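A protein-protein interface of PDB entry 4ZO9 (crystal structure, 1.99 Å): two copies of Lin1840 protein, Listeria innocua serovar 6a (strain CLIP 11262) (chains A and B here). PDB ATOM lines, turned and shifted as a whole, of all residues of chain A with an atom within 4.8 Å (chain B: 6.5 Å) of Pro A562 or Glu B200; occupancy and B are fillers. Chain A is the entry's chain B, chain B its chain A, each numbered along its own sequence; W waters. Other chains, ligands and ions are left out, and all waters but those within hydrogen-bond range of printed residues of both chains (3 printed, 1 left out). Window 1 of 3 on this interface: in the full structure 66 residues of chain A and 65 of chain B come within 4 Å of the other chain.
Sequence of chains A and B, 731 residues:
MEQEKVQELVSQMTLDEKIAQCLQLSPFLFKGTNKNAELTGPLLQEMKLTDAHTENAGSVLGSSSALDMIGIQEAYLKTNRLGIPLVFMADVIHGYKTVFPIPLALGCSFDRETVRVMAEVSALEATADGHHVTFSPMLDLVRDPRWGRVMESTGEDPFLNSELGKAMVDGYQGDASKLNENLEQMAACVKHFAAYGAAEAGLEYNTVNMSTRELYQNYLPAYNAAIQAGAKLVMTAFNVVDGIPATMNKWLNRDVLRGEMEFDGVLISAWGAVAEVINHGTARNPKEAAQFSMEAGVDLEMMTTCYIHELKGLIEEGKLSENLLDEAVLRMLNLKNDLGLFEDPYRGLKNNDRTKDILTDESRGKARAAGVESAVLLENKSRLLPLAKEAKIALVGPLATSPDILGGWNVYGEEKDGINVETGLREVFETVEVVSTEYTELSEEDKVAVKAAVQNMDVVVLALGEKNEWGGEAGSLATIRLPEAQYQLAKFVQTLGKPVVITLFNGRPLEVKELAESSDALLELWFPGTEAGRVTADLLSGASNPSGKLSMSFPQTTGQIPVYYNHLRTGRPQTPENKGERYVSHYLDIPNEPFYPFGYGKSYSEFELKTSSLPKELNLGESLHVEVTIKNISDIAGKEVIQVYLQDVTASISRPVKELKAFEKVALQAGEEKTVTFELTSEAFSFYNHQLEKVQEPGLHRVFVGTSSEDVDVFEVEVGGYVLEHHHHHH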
ATOM      1  N   ARG A 143      21.108  39.870  23.289  1.00  0.00           N
ATOM      2  CA  ARG A 143      20.971  38.939  22.121  1.00  0.00           C
ATOM      3  C   ARG A 143      19.572  38.889  21.489  1.00  0.00           C
ATOM      4  O   ARG A 143      19.311  38.070  20.578  1.00  0.00           O
ATOM      5  CB  ARG A 143      21.296  37.551  22.580  1.00  0.00           C
ATOM      6  CG  ARG A 143      22.674  37.451  23.189  1.00  0.00           C
ATOM      7  CD  ARG A 143      23.011  36.030  23.507  1.00  0.00           C
ATOM      8  NE  ARG A 143      24.407  35.830  23.677  1.00  0.00           N
ATOM      9  CZ  ARG A 143      24.954  34.755  24.240  1.00  0.00           C
ATOM     10  NH1 ARG A 143      24.205  33.782  24.706  1.00  0.00           N
ATOM     11  NH2 ARG A 143      26.275  34.676  24.346  1.00  0.00           N
ATOM     12  N   GLN A 560      14.565  33.689  14.013  1.00  0.00           N
ATOM     13  CA  GLN A 560      15.975  33.328  14.120  1.00  0.00           C
ATOM     14  C   GLN A 560      16.566  33.689  15.495  1.00  0.00           C
ATOM     15  O   GLN A 560      17.665  33.306  15.806  1.00  0.00           O
ATOM     16  CB  GLN A 560      16.791  34.067  13.053  1.00  0.00           C
ATOM     17  CG  GLN A 560      18.161  33.499  12.829  1.00  0.00           C
ATOM     18  CD  GLN A 560      18.871  34.129  11.653  1.00  0.00           C
ATOM     19  OE1 GLN A 560      19.012  35.356  11.543  1.00  0.00           O
ATOM     20  NE2 GLN A 560      19.375  33.300  10.826  1.00  0.00           N
ATOM     21  N   ILE A 561      15.832  34.470  16.281  1.00  0.00           N
ATOM     22  CA  ILE A 561      16.361  35.031  17.529  1.00  0.00           C
ATOM     23  C   ILE A 561      16.447  34.013  18.659  1.00  0.00           C
ATOM     24  O   ILE A 561      15.481  33.247  18.869  1.00  0.00           O
ATOM     25  CB  ILE A 561      15.417  36.175  18.003  1.00  0.00           C
ATOM     26  CG1 ILE A 561      15.501  37.342  17.052  1.00  0.00           C
ATOM     27  CG2 ILE A 561      15.787  36.604  19.402  1.00  0.00           C
ATOM     28  CD1 ILE A 561      14.397  38.369  17.254  1.00  0.00           C
ATOM     29  N   PRO A 562      17.548  34.003  19.435  1.00  0.00           N
ATOM     30  CA  PRO A 562      18.742  34.803  19.336  1.00  0.00           C
ATOM     31  C   PRO A 562      19.693  34.229  18.341  1.00  0.00           C
ATOM     32  O   PRO A 562      19.949  32.994  18.333  1.00  0.00           O
ATOM     33  CB  PRO A 562      19.322  34.707  20.754  1.00  0.00           C
ATOM     34  CG  PRO A 562      19.023  33.302  21.130  1.00  0.00           C
ATOM     35  CD  PRO A 562      17.616  33.126  20.624  1.00  0.00           C
ATOM     36  N   VAL A 563      20.247  35.130  17.542  1.00  0.00           N
ATOM     37  CA  VAL A 563      21.369  34.842  16.648  1.00  0.00           C
ATOM     38  C   VAL A 563      22.483  35.840  16.968  1.00  0.00           C
ATOM     39  O   VAL A 563      22.209  37.046  17.212  1.00  0.00           O
ATOM     40  CB  VAL A 563      20.950  34.937  15.160  1.00  0.00           C
ATOM     41  CG1 VAL A 563      20.342  36.279  14.828  1.00  0.00           C
ATOM     42  CG2 VAL A 563      22.122  34.582  14.253  1.00  0.00           C
ATOM     43  N   TYR A 564      23.713  35.356  17.003  1.00  0.00           N
ATOM     44  CA  TYR A 564      24.841  36.163  17.510  1.00  0.00           C
ATOM     45  C   TYR A 564      26.129  35.478  17.050  1.00  0.00           C
ATOM     46  O   TYR A 564      26.148  34.254  16.803  1.00  0.00           O
ATOM     47  CB  TYR A 564      24.772  36.384  19.063  1.00  0.00           C
ATOM     48  CG  TYR A 564      24.579  35.093  19.832  1.00  0.00           C
ATOM     49  CD1 TYR A 564      25.686  34.295  20.175  1.00  0.00           C
ATOM     50  CD2 TYR A 564      23.298  34.614  20.181  1.00  0.00           C
ATOM     51  CE1 TYR A 564      25.550  33.081  20.825  1.00  0.00           C
ATOM     52  CE2 TYR A 564      23.179  33.377  20.858  1.00  0.00           C
ATOM     53  CZ  TYR A 564      24.309  32.628  21.154  1.00  0.00           C
ATOM     54  OH  TYR A 564      24.236  31.400  21.788  1.00  0.00           O
ATOM     55  N   ASP B 144       9.135  25.390  22.681  1.00  0.00           N
ATOM     56  CA  ASP B 144       9.595  26.065  21.469  1.00  0.00           C
ATOM     57  C   ASP B 144       9.169  25.280  20.243  1.00  0.00           C
ATOM     58  O   ASP B 144       9.856  24.351  19.810  1.00  0.00           O
ATOM     59  CB  ASP B 144      11.105  26.330  21.503  1.00  0.00           C
ATOM     60  CG  ASP B 144      11.560  27.266  20.379  1.00  0.00           C
ATOM     61  OD1 ASP B 144      10.755  27.472  19.402  1.00  0.00           O
ATOM     62  OD2 ASP B 144      12.698  27.833  20.483  1.00  0.00           O
ATOM     63  N   ARG B 146       9.241  25.979  17.122  1.00  0.00           N
ATOM     64  CA  ARG B 146      10.161  26.010  15.986  1.00  0.00           C
ATOM     65  C   ARG B 146      10.845  24.670  15.818  1.00  0.00           C
ATOM     66  O   ARG B 146      11.079  24.211  14.686  1.00  0.00           O
ATOM     67  CB  ARG B 146      11.190  27.119  16.135  1.00  0.00           C
ATOM     68  CG  ARG B 146      10.546  28.495  15.992  1.00  0.00           C
ATOM     69  CD  ARG B 146      11.466  29.633  16.389  1.00  0.00           C
ATOM     70  NE  ARG B 146      11.819  29.640  17.807  1.00  0.00           N
ATOM     71  CZ  ARG B 146      12.519  30.582  18.412  1.00  0.00           C
ATOM     72  NH1 ARG B 146      12.989  31.606  17.763  1.00  0.00           N
ATOM     73  NH2 ARG B 146      12.752  30.486  19.692  1.00  0.00           N
ATOM     74  N   TYR B 196      17.239  18.373  25.698  1.00  0.00           N
ATOM     75  CA  TYR B 196      17.478  18.561  24.254  1.00  0.00           C
ATOM     76  C   TYR B 196      16.453  19.519  23.636  1.00  0.00           C
ATOM     77  O   TYR B 196      16.784  20.269  22.689  1.00  0.00           O
ATOM     78  CB  TYR B 196      17.422  17.102  23.586  1.00  0.00           C
ATOM     79  CG  TYR B 196      17.543  16.944  22.116  1.00  0.00           C
ATOM     80  CD1 TYR B 196      18.336  17.760  21.344  1.00  0.00           C
ATOM     81  CD2 TYR B 196      16.980  15.867  21.481  1.00  0.00           C
ATOM     82  CE1 TYR B 196      18.482  17.562  19.971  1.00  0.00           C
ATOM     83  CE2 TYR B 196      17.130  15.647  20.131  1.00  0.00           C
ATOM     84  CZ  TYR B 196      17.849  16.514  19.376  1.00  0.00           C
ATOM     85  OH  TYR B 196      17.973  16.356  18.037  1.00  0.00           O
ATOM     86  N   GLY B 197      15.206  19.443  24.141  1.00  0.00           N
ATOM     87  CA  GLY B 197      14.103  20.340  23.760  1.00  0.00           C
ATOM     88  C   GLY B 197      14.289  21.818  23.959  1.00  0.00           C
ATOM     89  O   GLY B 197      13.465  22.647  23.464  1.00  0.00           O
ATOM     90  N   ALA B 198      15.332  22.196  24.680  1.00  0.00           N
ATOM     91  CA  ALA B 198      15.527  23.624  24.959  1.00  0.00           C
ATOM     92  C   ALA B 198      16.472  24.258  23.929  1.00  0.00           C
ATOM     93  O   ALA B 198      16.980  25.356  24.135  1.00  0.00           O
ATOM     94  CB  ALA B 198      16.016  23.813  26.364  1.00  0.00           C
ATOM     95  N   ALA B 199      16.751  23.530  22.836  1.00  0.00           N
ATOM     96  CA  ALA B 199      17.597  24.023  21.761  1.00  0.00           C
ATOM     97  C   ALA B 199      17.340  25.487  21.460  1.00  0.00           C
ATOM     98  O   ALA B 199      16.160  25.930  21.232  1.00  0.00           O
ATOM     99  CB  ALA B 199      17.388  23.178  20.506  1.00  0.00           C
ATOM    100  N   GLU B 200      18.436  26.263  21.458  1.00  0.00           N
ATOM    101  CA  GLU B 200      18.311  27.726  21.355  1.00  0.00           C
ATOM    102  C   GLU B 200      17.709  28.055  19.954  1.00  0.00           C
ATOM    103  O   GLU B 200      18.030  27.411  18.970  1.00  0.00           O
ATOM    104  CB  GLU B 200      19.653  28.402  21.593  1.00  0.00           C
ATOM    105  CG  GLU B 200      19.638  29.921  21.730  1.00  0.00           C
ATOM    106  CD  GLU B 200      20.909  30.431  22.389  1.00  0.00           C
ATOM    107  OE1 GLU B 200      21.797  30.723  21.561  1.00  0.00           O
ATOM    108  OE2 GLU B 200      21.013  30.501  23.689  1.00  0.00           O
ATOM    109  N   ALA B 201      16.741  28.973  19.937  1.00  0.00           N
ATOM    110  CA  ALA B 201      16.093  29.471  18.700  1.00  0.00           C
ATOM    111  C   ALA B 201      15.368  28.388  17.927  1.00  0.00           C
ATOM    112  O   ALA B 201      15.074  28.573  16.758  1.00  0.00           O
ATOM    113  CB  ALA B 201      17.130  30.136  17.781  1.00  0.00           C
ATOM    114  N   GLY B 202      15.097  27.267  18.581  1.00  0.00           N
ATOM    115  CA  GLY B 202      14.459  26.105  17.984  1.00  0.00           C
ATOM    116  C   GLY B 202      15.265  25.414  16.896  1.00  0.00           C
ATOM    117  O   GLY B 202      14.732  24.665  16.106  1.00  0.00           O
ATOM    118  N   LEU B 203      16.545  25.706  16.852  1.00  0.00           N
ATOM    119  CA  LEU B 203      17.456  25.193  15.823  1.00  0.00           C
ATOM    120  C   LEU B 203      17.978  23.786  16.143  1.00  0.00           C
ATOM    121  O   LEU B 203      18.433  23.509  17.226  1.00  0.00           O
ATOM    122  CB  LEU B 203      18.623  26.174  15.644  1.00  0.00           C
ATOM    123  CG  LEU B 203      19.657  25.819  14.597  1.00  0.00           C
ATOM    124  CD1 LEU B 203      18.991  25.630  13.241  1.00  0.00           C
ATOM    125  CD2 LEU B 203      20.735  26.908  14.537  1.00  0.00           C
ATOM    126  N   GLU B 204      17.895  22.860  15.203  1.00  0.00           N
ATOM    127  CA  GLU B 204      18.294  21.532  15.523  1.00  0.00           C
ATOM    128  C   GLU B 204      19.740  21.457  16.009  1.00  0.00           C
ATOM    129  O   GLU B 204      20.685  22.035  15.409  1.00  0.00           O
ATOM    130  CB  GLU B 204      18.050  20.599  14.310  1.00  0.00           C
ATOM    131  CG  GLU B 204      18.091  19.195  14.641  1.00  0.00           C
ATOM    132  CD  GLU B 204      17.047  18.816  15.643  1.00  0.00           C
ATOM    133  OE1 GLU B 204      15.869  18.583  15.289  1.00  0.00           O
ATOM    134  OE2 GLU B 204      17.413  18.713  16.818  1.00  0.00           O
ATOM    135  N   ASN B 206      21.113  22.624  18.552  1.00  0.00           N
ATOM    136  CA  ASN B 206      21.717  23.864  18.984  1.00  0.00           C
ATOM    137  C   ASN B 206      21.886  23.923  20.510  1.00  0.00           C
ATOM    138  O   ASN B 206      21.274  23.135  21.240  1.00  0.00           O
ATOM    139  CB  ASN B 206      20.936  25.057  18.457  1.00  0.00           C
ATOM    140  CG  ASN B 206      21.768  26.310  18.384  1.00  0.00           C
ATOM    141  OD1 ASN B 206      23.034  26.274  18.343  1.00  0.00           O
ATOM    142  ND2 ASN B 206      21.068  27.463  18.385  1.00  0.00           N
ATOM    143  N   THR B 207      22.750  24.840  20.945  1.00  0.00           N
ATOM    144  CA  THR B 207      23.009  25.148  22.317  1.00  0.00           C
ATOM    145  C   THR B 207      21.805  25.141  23.249  1.00  0.00           C
ATOM    146  O   THR B 207      20.748  25.691  22.974  1.00  0.00           O
ATOM    147  CB  THR B 207      23.626  26.528  22.378  1.00  0.00           C
ATOM    148  OG1 THR B 207      24.797  26.520  21.554  1.00  0.00           O
ATOM    149  CG2 THR B 207      23.925  26.955  23.801  1.00  0.00           C
ATOM    150  N   VAL B 208      21.991  24.458  24.366  1.00  0.00           N
ATOM    151  CA  VAL B 208      21.041  24.483  25.473  1.00  0.00           C
ATOM    152  C   VAL B 208      21.794  25.049  26.667  1.00  0.00           C
ATOM    153  O   VAL B 208      22.988  24.706  26.901  1.00  0.00           O
ATOM    154  CB  VAL B 208      20.544  23.069  25.813  1.00  0.00           C
ATOM    155  CG1 VAL B 208      19.778  23.092  27.136  1.00  0.00           C
ATOM    156  CG2 VAL B 208      19.690  22.472  24.670  1.00  0.00           C
ATOM    157  N   ASN B 209      21.119  25.922  27.391  1.00  0.00           N
ATOM    158  CA  ASN B 209      21.652  26.485  28.638  1.00  0.00           C
ATOM    159  C   ASN B 209      20.496  26.900  29.518  1.00  0.00           C
ATOM    160  O   ASN B 209      19.568  27.540  29.045  1.00  0.00           O
ATOM    161  CB  ASN B 209      22.583  27.672  28.402  1.00  0.00           C
ATOM    162  CG  ASN B 209      23.285  28.118  29.674  1.00  0.00           C
ATOM    163  OD1 ASN B 209      22.847  29.068  30.311  1.00  0.00           O
ATOM    164  ND2 ASN B 209      24.337  27.395  30.084  1.00  0.00           N
HETATM  165  O   HOH W   1      21.610  33.101  24.065  1.00  0.00           O
HETATM  166  O   HOH W   2      25.375  28.836  20.785  1.00  0.00           O
HETATM  167  O   HOH W   3      21.114  30.439  17.185  1.00  0.00           O
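The side-chain carboxylate of Glu B200 sits at hydrogen-bond distance from the side-chain hydroxyl of Tyr A564, at 2.5 Å. O of Ile A561 lies within hydrogen-bond range of NH1 of Arg B146 (3.2 Å).
The side-chain carboxylate (OD2) of Asp B144 is in salt-bridge range of the guanidinium group (NH2) of Arg B146 (2.8 Å). O of Glu B200 is in hydrogen-bond range of ND2 of Asn B206, 3.1 Å away. The backbone NH of Glu B200 lies within hydrogen-bond range of the backbone carbonyl oxygen of Thr B207 (2.8 Å).
Gln A560 touches Ala B201. Ile A561 touches Ala B201. Pro A562 touches Glu B200.
Of the printed residues of chain B, Gln A560 touches Ala B201 (3.8 Å). Printed residues of chain B within 4 Å of Ile A561: Arg B146 (3.2 Å) and Ala B201 (3.7 Å). Of chain B, only Glu B200 comes within 4 Å of Pro A562. Printed residues of chain A within 4 Å of Arg B146: Ile A561. Of chain A, only Pro A562 and Tyr A564 come within 4 Å of Glu B200. The nearest printed residue of chain B that does not touch Ile A561 is Glu B200 (5.8 Å).
Of the 6 printed residues of chain A, 4 touch a printed residue of chain B. Hydrophobic or aromatic side chains of chain A that line the printed part of chain B: Pro A562 and Tyr A564. Among the printed residues, 5 pairs touch across the chains.
No position is printed for both chains.
Water W2 lies within hydrogen-bond range of OG1 of Thr B207 and OH of Tyr A564. Water W1 bridges OE2 of Glu B200 (2.7 Å) and NH1 of Arg A143 (2.8 Å). Water W3 lies within hydrogen-bond range of the backbone carbonyl oxygen of Pro A562 (3.0 Å) and the side-chain amide nitrogen of Asn B206 (3.2 Å).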
